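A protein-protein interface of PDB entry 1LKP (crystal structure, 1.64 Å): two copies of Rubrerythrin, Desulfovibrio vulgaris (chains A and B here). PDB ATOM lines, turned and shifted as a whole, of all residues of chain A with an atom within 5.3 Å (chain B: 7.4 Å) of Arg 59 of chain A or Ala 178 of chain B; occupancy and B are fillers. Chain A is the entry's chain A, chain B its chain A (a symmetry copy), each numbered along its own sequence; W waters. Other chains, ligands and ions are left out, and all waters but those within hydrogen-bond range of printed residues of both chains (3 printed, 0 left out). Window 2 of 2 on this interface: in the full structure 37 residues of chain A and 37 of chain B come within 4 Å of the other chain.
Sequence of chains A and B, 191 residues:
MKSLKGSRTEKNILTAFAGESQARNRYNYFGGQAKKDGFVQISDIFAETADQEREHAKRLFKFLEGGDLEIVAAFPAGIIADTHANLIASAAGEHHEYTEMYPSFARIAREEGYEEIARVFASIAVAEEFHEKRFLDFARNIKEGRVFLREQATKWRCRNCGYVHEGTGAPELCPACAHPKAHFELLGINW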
ATOM      1  N   ARG A  54      20.524  25.105  -9.139  1.00  0.00           N
ATOM      2  CA  ARG A  54      19.173  25.585  -9.401  1.00  0.00           C
ATOM      3  C   ARG A  54      18.548  24.688 -10.463  1.00  0.00           C
ATOM      4  O   ARG A  54      17.361  24.368 -10.403  1.00  0.00           O
ATOM      5  CB  ARG A  54      19.204  27.032  -9.909  1.00  0.00           C
ATOM      6  CG  ARG A  54      17.849  27.603 -10.336  1.00  0.00           C
ATOM      7  CD  ARG A  54      18.069  28.871 -11.153  1.00  0.00           C
ATOM      8  NE  ARG A  54      18.861  28.567 -12.339  1.00  0.00           N
ATOM      9  CZ  ARG A  54      19.608  29.441 -13.003  1.00  0.00           C
ATOM     10  NH1 ARG A  54      19.676  30.707 -12.607  1.00  0.00           N
ATOM     11  NH2 ARG A  54      20.303  29.039 -14.059  1.00  0.00           N
ATOM     12  N   GLU A  55      19.362  24.277 -11.432  1.00  0.00           N
ATOM     13  CA  GLU A  55      18.884  23.424 -12.514  1.00  0.00           C
ATOM     14  C   GLU A  55      18.655  21.975 -12.074  1.00  0.00           C
ATOM     15  O   GLU A  55      17.753  21.312 -12.579  1.00  0.00           O
ATOM     16  CB  GLU A  55      19.849  23.507 -13.697  1.00  0.00           C
ATOM     17  CG  GLU A  55      19.909  24.913 -14.317  1.00  0.00           C
ATOM     18  CD  GLU A  55      18.551  25.403 -14.808  1.00  0.00           C
ATOM     19  OE1 GLU A  55      17.851  24.628 -15.489  1.00  0.00           O
ATOM     20  OE2 GLU A  55      18.186  26.568 -14.527  1.00  0.00           O
ATOM     21  N   HIS A  56      19.465  21.475 -11.146  1.00  0.00           N
ATOM     22  CA  HIS A  56      19.247  20.117 -10.642  1.00  0.00           C
ATOM     23  C   HIS A  56      17.893  20.149  -9.929  1.00  0.00           C
ATOM     24  O   HIS A  56      17.059  19.260 -10.098  1.00  0.00           O
ATOM     25  CB  HIS A  56      20.306  19.725  -9.608  1.00  0.00           C
ATOM     26  CG  HIS A  56      21.693  19.627 -10.157  1.00  0.00           C
ATOM     27  ND1 HIS A  56      22.801  19.504  -9.348  1.00  0.00           N
ATOM     28  CD2 HIS A  56      22.154  19.648 -11.430  1.00  0.00           C
ATOM     29  CE1 HIS A  56      23.888  19.458 -10.099  1.00  0.00           C
ATOM     30  NE2 HIS A  56      23.523  19.543 -11.366  1.00  0.00           N
ATOM     31  N   ALA A  57      17.696  21.188  -9.120  1.00  0.00           N
ATOM     32  CA  ALA A  57      16.464  21.351  -8.363  1.00  0.00           C
ATOM     33  C   ALA A  57      15.251  21.455  -9.275  1.00  0.00           C
ATOM     34  O   ALA A  57      14.205  20.882  -8.988  1.00  0.00           O
ATOM     35  CB  ALA A  57      16.552  22.591  -7.465  1.00  0.00           C
ATOM     36  N   LYS A  58      15.389  22.182 -10.379  1.00  0.00           N
ATOM     37  CA  LYS A  58      14.273  22.344 -11.307  1.00  0.00           C
ATOM     38  C   LYS A  58      13.854  21.012 -11.919  1.00  0.00           C
ATOM     39  O   LYS A  58      12.661  20.729 -12.034  1.00  0.00           O
ATOM     40  CB  LYS A  58      14.635  23.325 -12.418  1.00  0.00           C
ATOM     41  CG  LYS A  58      13.446  23.750 -13.268  1.00  0.00           C
ATOM     42  CD  LYS A  58      13.874  24.725 -14.348  1.00  0.00           C
ATOM     43  CE  LYS A  58      12.682  25.208 -15.160  1.00  0.00           C
ATOM     44  NZ  LYS A  58      13.098  26.204 -16.191  1.00  0.00           N
ATOM     45  N   ARG A  59      14.833  20.205 -12.318  1.00  0.00           N
ATOM     46  CA  ARG A  59      14.543  18.903 -12.911  1.00  0.00           C
ATOM     47  C   ARG A  59      13.790  18.048 -11.899  1.00  0.00           C
ATOM     48  O   ARG A  59      12.800  17.401 -12.232  1.00  0.00           O
ATOM     49  CB  ARG A  59      15.838  18.190 -13.325  1.00  0.00           C
ATOM     50  CG  ARG A  59      15.614  16.850 -14.046  1.00  0.00           C
ATOM     51  CD  ARG A  59      15.017  17.073 -15.434  1.00  0.00           C
ATOM     52  NE  ARG A  59      14.404  15.875 -16.013  1.00  0.00           N
ATOM     53  CZ  ARG A  59      15.054  14.920 -16.673  1.00  0.00           C
ATOM     54  NH1 ARG A  59      16.366  14.996 -16.855  1.00  0.00           N
ATOM     55  NH2 ARG A  59      14.383  13.889 -17.172  1.00  0.00           N
ATOM     56  N   LEU A  60      14.263  18.056 -10.656  1.00  0.00           N
ATOM     57  CA  LEU A  60      13.635  17.279  -9.596  1.00  0.00           C
ATOM     58  C   LEU A  60      12.236  17.792  -9.297  1.00  0.00           C
ATOM     59  O   LEU A  60      11.287  17.015  -9.178  1.00  0.00           O
ATOM     60  CB  LEU A  60      14.491  17.345  -8.327  1.00  0.00           C
ATOM     61  CG  LEU A  60      15.875  16.706  -8.443  1.00  0.00           C
ATOM     62  CD1 LEU A  60      16.754  17.141  -7.279  1.00  0.00           C
ATOM     63  CD2 LEU A  60      15.722  15.191  -8.485  1.00  0.00           C
ATOM     64  N   PHE A  61      12.112  19.108  -9.185  1.00  0.00           N
ATOM     65  CA  PHE A  61      10.836  19.741  -8.886  1.00  0.00           C
ATOM     66  C   PHE A  61       9.760  19.353  -9.900  1.00  0.00           C
ATOM     67  O   PHE A  61       8.617  19.088  -9.529  1.00  0.00           O
ATOM     68  CB  PHE A  61      11.007  21.263  -8.872  1.00  0.00           C
ATOM     69  CG  PHE A  61       9.833  22.007  -8.292  1.00  0.00           C
ATOM     70  CD1 PHE A  61       9.547  21.933  -6.930  1.00  0.00           C
ATOM     71  CD2 PHE A  61       9.022  22.793  -9.106  1.00  0.00           C
ATOM     72  CE1 PHE A  61       8.470  22.634  -6.387  1.00  0.00           C
ATOM     73  CE2 PHE A  61       7.939  23.499  -8.574  1.00  0.00           C
ATOM     74  CZ  PHE A  61       7.664  23.419  -7.214  1.00  0.00           C
ATOM     75  N   LYS A  62      10.137  19.309 -11.173  1.00  0.00           N
ATOM     76  CA  LYS A  62       9.197  18.980 -12.237  1.00  0.00           C
ATOM     77  C   LYS A  62       8.632  17.558 -12.208  1.00  0.00           C
ATOM     78  O   LYS A  62       7.614  17.288 -12.846  1.00  0.00           O
ATOM     79  CB  LYS A  62       9.836  19.285 -13.596  1.00  0.00           C
ATOM     80  CG  LYS A  62      10.046  20.783 -13.815  1.00  0.00           C
ATOM     81  CD  LYS A  62      10.692  21.099 -15.153  1.00  0.00           C
ATOM     82  CE  LYS A  62       9.788  20.720 -16.317  1.00  0.00           C
ATOM     83  NZ  LYS A  62      10.362  21.158 -17.617  1.00  0.00           N
ATOM     84  N   PHE A  63       9.277  16.656 -11.471  1.00  0.00           N
ATOM     85  CA  PHE A  63       8.790  15.280 -11.365  1.00  0.00           C
ATOM     86  C   PHE A  63       7.639  15.174 -10.371  1.00  0.00           C
ATOM     87  O   PHE A  63       6.788  14.291 -10.484  1.00  0.00           O
ATOM     88  CB  PHE A  63       9.904  14.332 -10.904  1.00  0.00           C
ATOM     89  CG  PHE A  63      10.895  13.979 -11.974  1.00  0.00           C
ATOM     90  CD1 PHE A  63      10.470  13.437 -13.184  1.00  0.00           C
ATOM     91  CD2 PHE A  63      12.257  14.158 -11.764  1.00  0.00           C
ATOM     92  CE1 PHE A  63      11.390  13.079 -14.169  1.00  0.00           C
ATOM     93  CE2 PHE A  63      13.183  13.802 -12.744  1.00  0.00           C
ATOM     94  CZ  PHE A  63      12.748  13.261 -13.947  1.00  0.00           C
ATOM     95  N   GLU A 116      13.449   6.310 -15.151  1.00  0.00           N
ATOM     96  CA  GLU A 116      13.844   7.631 -15.625  1.00  0.00           C
ATOM     97  C   GLU A 116      14.404   8.456 -14.477  1.00  0.00           C
ATOM     98  O   GLU A 116      15.479   9.047 -14.589  1.00  0.00           O
ATOM     99  CB  GLU A 116      12.649   8.360 -16.243  1.00  0.00           C
ATOM    100  CG  GLU A 116      12.986   9.746 -16.773  1.00  0.00           C
ATOM    101  CD  GLU A 116      11.785  10.460 -17.364  1.00  0.00           C
ATOM    102  OE1 GLU A 116      11.952  11.595 -17.858  1.00  0.00           O
ATOM    103  OE2 GLU A 116      10.674   9.888 -17.331  1.00  0.00           O
ATOM    104  N   VAL A 120      18.154  10.040 -13.664  1.00  0.00           N
ATOM    105  CA  VAL A 120      18.387  11.445 -13.372  1.00  0.00           C
ATOM    106  C   VAL A 120      19.221  11.590 -12.103  1.00  0.00           C
ATOM    107  O   VAL A 120      20.149  12.392 -12.062  1.00  0.00           O
ATOM    108  CB  VAL A 120      17.057  12.209 -13.214  1.00  0.00           C
ATOM    109  CG1 VAL A 120      17.318  13.621 -12.714  1.00  0.00           C
ATOM    110  CG2 VAL A 120      16.333  12.255 -14.553  1.00  0.00           C
ATOM    111  N   CYS B 158      27.951  19.990 -19.515  1.00  0.00           N
ATOM    112  CA  CYS B 158      26.699  20.697 -19.764  1.00  0.00           C
ATOM    113  C   CYS B 158      26.800  22.017 -19.002  1.00  0.00           C
ATOM    114  O   CYS B 158      26.917  22.020 -17.779  1.00  0.00           O
ATOM    115  CB  CYS B 158      25.512  19.892 -19.230  1.00  0.00           C
ATOM    116  SG  CYS B 158      23.938  20.780 -19.305  1.00  0.00           S
ATOM    117  N   ASN B 160      24.512  24.101 -18.459  1.00  0.00           N
ATOM    118  CA  ASN B 160      23.307  24.325 -17.664  1.00  0.00           C
ATOM    119  C   ASN B 160      23.318  23.684 -16.275  1.00  0.00           C
ATOM    120  O   ASN B 160      22.891  24.314 -15.297  1.00  0.00           O
ATOM    121  CB  ASN B 160      22.066  23.838 -18.422  1.00  0.00           C
ATOM    122  CG  ASN B 160      20.771  24.245 -17.740  1.00  0.00           C
ATOM    123  OD1 ASN B 160      20.000  23.397 -17.276  1.00  0.00           O
ATOM    124  ND2 ASN B 160      20.526  25.549 -17.672  1.00  0.00           N
ATOM    125  N   CYS B 161      23.809  22.449 -16.177  1.00  0.00           N
ATOM    126  CA  CYS B 161      23.808  21.748 -14.891  1.00  0.00           C
ATOM    127  C   CYS B 161      25.130  21.127 -14.450  1.00  0.00           C
ATOM    128  O   CYS B 161      25.220  20.590 -13.345  1.00  0.00           O
ATOM    129  CB  CYS B 161      22.739  20.656 -14.893  1.00  0.00           C
ATOM    130  SG  CYS B 161      23.207  19.185 -15.846  1.00  0.00           S
ATOM    131  N   GLU B 172      22.415  14.494 -27.498  1.00  0.00           N
ATOM    132  CA  GLU B 172      21.298  15.286 -28.001  1.00  0.00           C
ATOM    133  C   GLU B 172      20.558  15.970 -26.861  1.00  0.00           C
ATOM    134  O   GLU B 172      20.045  17.076 -27.014  1.00  0.00           O
ATOM    135  CB  GLU B 172      20.325  14.400 -28.781  1.00  0.00           C
ATOM    136  CG  GLU B 172      20.900  13.866 -30.078  1.00  0.00           C
ATOM    137  CD  GLU B 172      21.342  14.978 -31.009  1.00  0.00           C
ATOM    138  OE1 GLU B 172      20.483  15.782 -31.426  1.00  0.00           O
ATOM    139  OE2 GLU B 172      22.547  15.051 -31.322  1.00  0.00           O
ATOM    140  N   LEU B 173      20.499  15.290 -25.721  1.00  0.00           N
ATOM    141  CA  LEU B 173      19.840  15.816 -24.532  1.00  0.00           C
ATOM    142  C   LEU B 173      20.672  15.463 -23.309  1.00  0.00           C
ATOM    143  O   LEU B 173      21.198  14.355 -23.209  1.00  0.00           O
ATOM    144  CB  LEU B 173      18.441  15.211 -24.377  1.00  0.00           C
ATOM    145  CG  LEU B 173      17.353  15.652 -25.356  1.00  0.00           C
ATOM    146  CD1 LEU B 173      16.063  14.901 -25.048  1.00  0.00           C
ATOM    147  CD2 LEU B 173      17.131  17.154 -25.241  1.00  0.00           C
ATOM    148  N   CYS B 174      20.799  16.407 -22.383  1.00  0.00           N
ATOM    149  CA  CYS B 174      21.560  16.154 -21.167  1.00  0.00           C
ATOM    150  C   CYS B 174      20.780  15.155 -20.315  1.00  0.00           C
ATOM    151  O   CYS B 174      19.605  15.364 -20.018  1.00  0.00           O
ATOM    152  CB  CYS B 174      21.766  17.454 -20.387  1.00  0.00           C
ATOM    153  SG  CYS B 174      22.640  17.215 -18.824  1.00  0.00           S
ATOM    154  N   PRO B 175      21.419  14.047 -19.920  1.00  0.00           N
ATOM    155  CA  PRO B 175      20.699  13.066 -19.104  1.00  0.00           C
ATOM    156  C   PRO B 175      20.323  13.547 -17.703  1.00  0.00           C
ATOM    157  O   PRO B 175      19.471  12.948 -17.042  1.00  0.00           O
ATOM    158  CB  PRO B 175      21.651  11.873 -19.080  1.00  0.00           C
ATOM    159  CG  PRO B 175      22.991  12.519 -19.154  1.00  0.00           C
ATOM    160  CD  PRO B 175      22.789  13.589 -20.212  1.00  0.00           C
ATOM    161  N   ALA B 176      20.956  14.625 -17.251  1.00  0.00           N
ATOM    162  CA  ALA B 176      20.666  15.170 -15.930  1.00  0.00           C
ATOM    163  C   ALA B 176      19.566  16.231 -15.949  1.00  0.00           C
ATOM    164  O   ALA B 176      18.539  16.075 -15.293  1.00  0.00           O
ATOM    165  CB  ALA B 176      21.936  15.755 -15.313  1.00  0.00           C
ATOM    166  N   CYS B 177      19.769  17.301 -16.713  1.00  0.00           N
ATOM    167  CA  CYS B 177      18.792  18.390 -16.756  1.00  0.00           C
ATOM    168  C   CYS B 177      17.857  18.423 -17.966  1.00  0.00           C
ATOM    169  O   CYS B 177      16.999  19.303 -18.062  1.00  0.00           O
ATOM    170  CB  CYS B 177      19.507  19.739 -16.645  1.00  0.00           C
ATOM    171  SG  CYS B 177      20.412  20.210 -18.138  1.00  0.00           S
ATOM    172  N   ALA B 178      18.034  17.485 -18.888  1.00  0.00           N
ATOM    173  CA  ALA B 178      17.192  17.390 -20.078  1.00  0.00           C
ATOM    174  C   ALA B 178      17.288  18.556 -21.060  1.00  0.00           C
ATOM    175  O   ALA B 178      16.445  18.687 -21.951  1.00  0.00           O
ATOM    176  CB  ALA B 178      15.728  17.179 -19.667  1.00  0.00           C
ATOM    177  N   HIS B 179      18.289  19.414 -20.905  1.00  0.00           N
ATOM    178  CA  HIS B 179      18.440  20.519 -21.845  1.00  0.00           C
ATOM    179  C   HIS B 179      19.137  20.006 -23.103  1.00  0.00           C
ATOM    180  O   HIS B 179      19.835  18.995 -23.066  1.00  0.00           O
ATOM    181  CB  HIS B 179      19.205  21.672 -21.202  1.00  0.00           C
ATOM    182  CG  HIS B 179      18.356  22.510 -20.298  1.00  0.00           C
ATOM    183  ND1 HIS B 179      17.608  21.970 -19.272  1.00  0.00           N
ATOM    184  CD2 HIS B 179      18.112  23.841 -20.280  1.00  0.00           C
ATOM    185  CE1 HIS B 179      16.940  22.934 -18.663  1.00  0.00           C
ATOM    186  NE2 HIS B 179      17.228  24.078 -19.255  1.00  0.00           N
ATOM    187  N   PRO B 180      18.946  20.691 -24.240  1.00  0.00           N
ATOM    188  CA  PRO B 180      19.563  20.267 -25.500  1.00  0.00           C
ATOM    189  C   PRO B 180      21.076  20.365 -25.624  1.00  0.00           C
ATOM    190  O   PRO B 180      21.741  21.068 -24.863  1.00  0.00           O
ATOM    191  CB  PRO B 180      18.838  21.121 -26.540  1.00  0.00           C
ATOM    192  CG  PRO B 180      18.554  22.378 -25.801  1.00  0.00           C
ATOM    193  CD  PRO B 180      18.107  21.888 -24.440  1.00  0.00           C
ATOM    194  N   LYS B 181      21.595  19.629 -26.604  1.00  0.00           N
ATOM    195  CA  LYS B 181      23.015  19.566 -26.925  1.00  0.00           C
ATOM    196  C   LYS B 181      23.660  20.950 -26.928  1.00  0.00           C
ATOM    197  O   LYS B 181      24.837  21.105 -26.596  1.00  0.00           O
ATOM    198  CB  LYS B 181      23.173  18.911 -28.303  1.00  0.00           C
ATOM    199  CG  LYS B 181      24.600  18.792 -28.810  1.00  0.00           C
ATOM    200  CD  LYS B 181      24.649  17.992 -30.110  1.00  0.00           C
ATOM    201  CE  LYS B 181      23.864  18.670 -31.225  1.00  0.00           C
ATOM    202  NZ  LYS B 181      23.855  17.847 -32.473  1.00  0.00           N
ATOM    203  N   HIS B 183      23.778  23.238 -24.983  1.00  0.00           N
ATOM    204  CA  HIS B 183      24.405  23.648 -23.731  1.00  0.00           C
ATOM    205  C   HIS B 183      25.773  23.035 -23.446  1.00  0.00           C
ATOM    206  O   HIS B 183      26.446  23.438 -22.498  1.00  0.00           O
ATOM    207  CB  HIS B 183      23.456  23.345 -22.571  1.00  0.00           C
ATOM    208  CG  HIS B 183      22.217  24.181 -22.579  1.00  0.00           C
ATOM    209  ND1 HIS B 183      22.108  25.356 -21.865  1.00  0.00           N
ATOM    210  CD2 HIS B 183      21.058  24.047 -23.265  1.00  0.00           C
ATOM    211  CE1 HIS B 183      20.933  25.910 -22.113  1.00  0.00           C
ATOM    212  NE2 HIS B 183      20.278  25.136 -22.960  1.00  0.00           N
HETATM  213  O   HOH W   1      17.172  13.829 -19.371  1.00  0.00           O
HETATM  214  O   HOH W   2      15.936  25.558 -17.204  1.00  0.00           O
HETATM  215  O   HOH W   3      22.752  27.084 -15.065  1.00  0.00           O
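The side-chain amide oxygen (OD1) of Asn 160 of chain B lies close to the side-chain carboxylate (OE1) of Glu 55 of chain A (3.1 Å). NE2 of His 56 of chain A sits at hydrogen-bond distance from O of Cys 161 of chain B. The guanidinium group (NH1) of Arg 59 of chain A lies within hydrogen-bond range of the backbone carbonyl oxygen (O) of Ala 176 of chain B, 2.9 Å away.
The side-chain carboxylate (OE2) of Glu 55 of chain A lies within salt-bridge range of the guanidinium group (NE) of Arg 54 of chain A (3.0 Å). The side-chain amide oxygen (OD1) of Asn 160 of chain B lies close to the side-chain sulfur (SG) of Cys 177 of chain B, at 3.3 Å. ND1 of His 179 of chain B sits close to OD1 of Asn 160 of chain B (3.4 Å). The side-chain sulfur of Cys 174 of chain B lies close to the backbone NH of Ala 176 of chain B (3.5 Å). N of Cys 174 of chain B lies within hydrogen-bond range of O of His 179 of chain B. ND1 of His 179 of chain B lies within hydrogen-bond range of O of Cys 177 of chain B (3.0 Å).
Glu 55 of chain A touches His 179 of chain B (OE1 to CE1, 3.7 Å). O of Pro 175 of chain B touches NH1 of Arg 59 of chain A (3.7 Å). Cys 177 of chain B touches Arg 59 of chain A. NH1 of Arg 59 of chain A touches CB of Ala 178 of chain B, 3.6 Å away. Ala 176 of chain B touches Val 120 of chain A.
Printed residues of chain B within 4 Å of Arg 59 of chain A: Pro 175 (3.7 Å), Ala 176 (2.9 Å), Cys 177 (3.9 Å) and Ala 178 (3.6 Å). Printed residues of chain A within 4 Å of Ala 178 of chain B: Arg 59 (3.6 Å). Of the printed residues of chain B, His 56 of chain A touches Cys 161 (2.8 Å). Of the printed residues of chain A, His 179 of chain B touches Glu 55. Of the printed residues of chain A, Cys 177 of chain B touches Arg 59. Printed residues of chain A within 4 Å of Pro 175 of chain B: Arg 59 (3.7 Å). Printed residues of chain A within 4 Å of Cys 161 of chain B: His 56. Lys 62 of chain A touches none of the printed residues of chain B. The nearest printed residue of chain A that does not touch Ala 178 of chain B is Glu 116 of chain A (7.0 Å).
Printed residues of chain B that touch a printed residue of chain A: Asn 160, Cys 161, Pro 175, Ala 176, Cys 177, Ala 178 and His 179. Hydrophobic or aromatic side chains of chain A within 4 Å of the printed part of chain B: His 56 and Val 120. Among the printed residues, 8 pairs touch across the chains. Among the printed residues, no Asp or Glu carboxylate lies within 4 Å of a Lys or Arg side-chain nitrogen of the other chain.
No position is printed for both chains. Of the 8 pairs that touch across the chains among the printed residues, none has its exchanged pair printed and touching as well.
Water W2 lies within hydrogen-bond range of the side-chain carboxylate (OE1) of Glu 55 of chain A, a ring nitrogen (NE2) of His 179 of chain B and the side-chain amino group (NZ) of Lys 58 of chain A. Water W3 lies within hydrogen-bond range of O of Asn 160 of chain B (2.8 Å) and NH2 of Arg 54 of chain A (3.3 Å). Water W1 lies within hydrogen-bond range of NH1 of Arg 59 of chain A (2.9 Å), O of Cys 174 of chain B (2.9 Å) and O of Pro 175 of chain B (3.4 Å).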
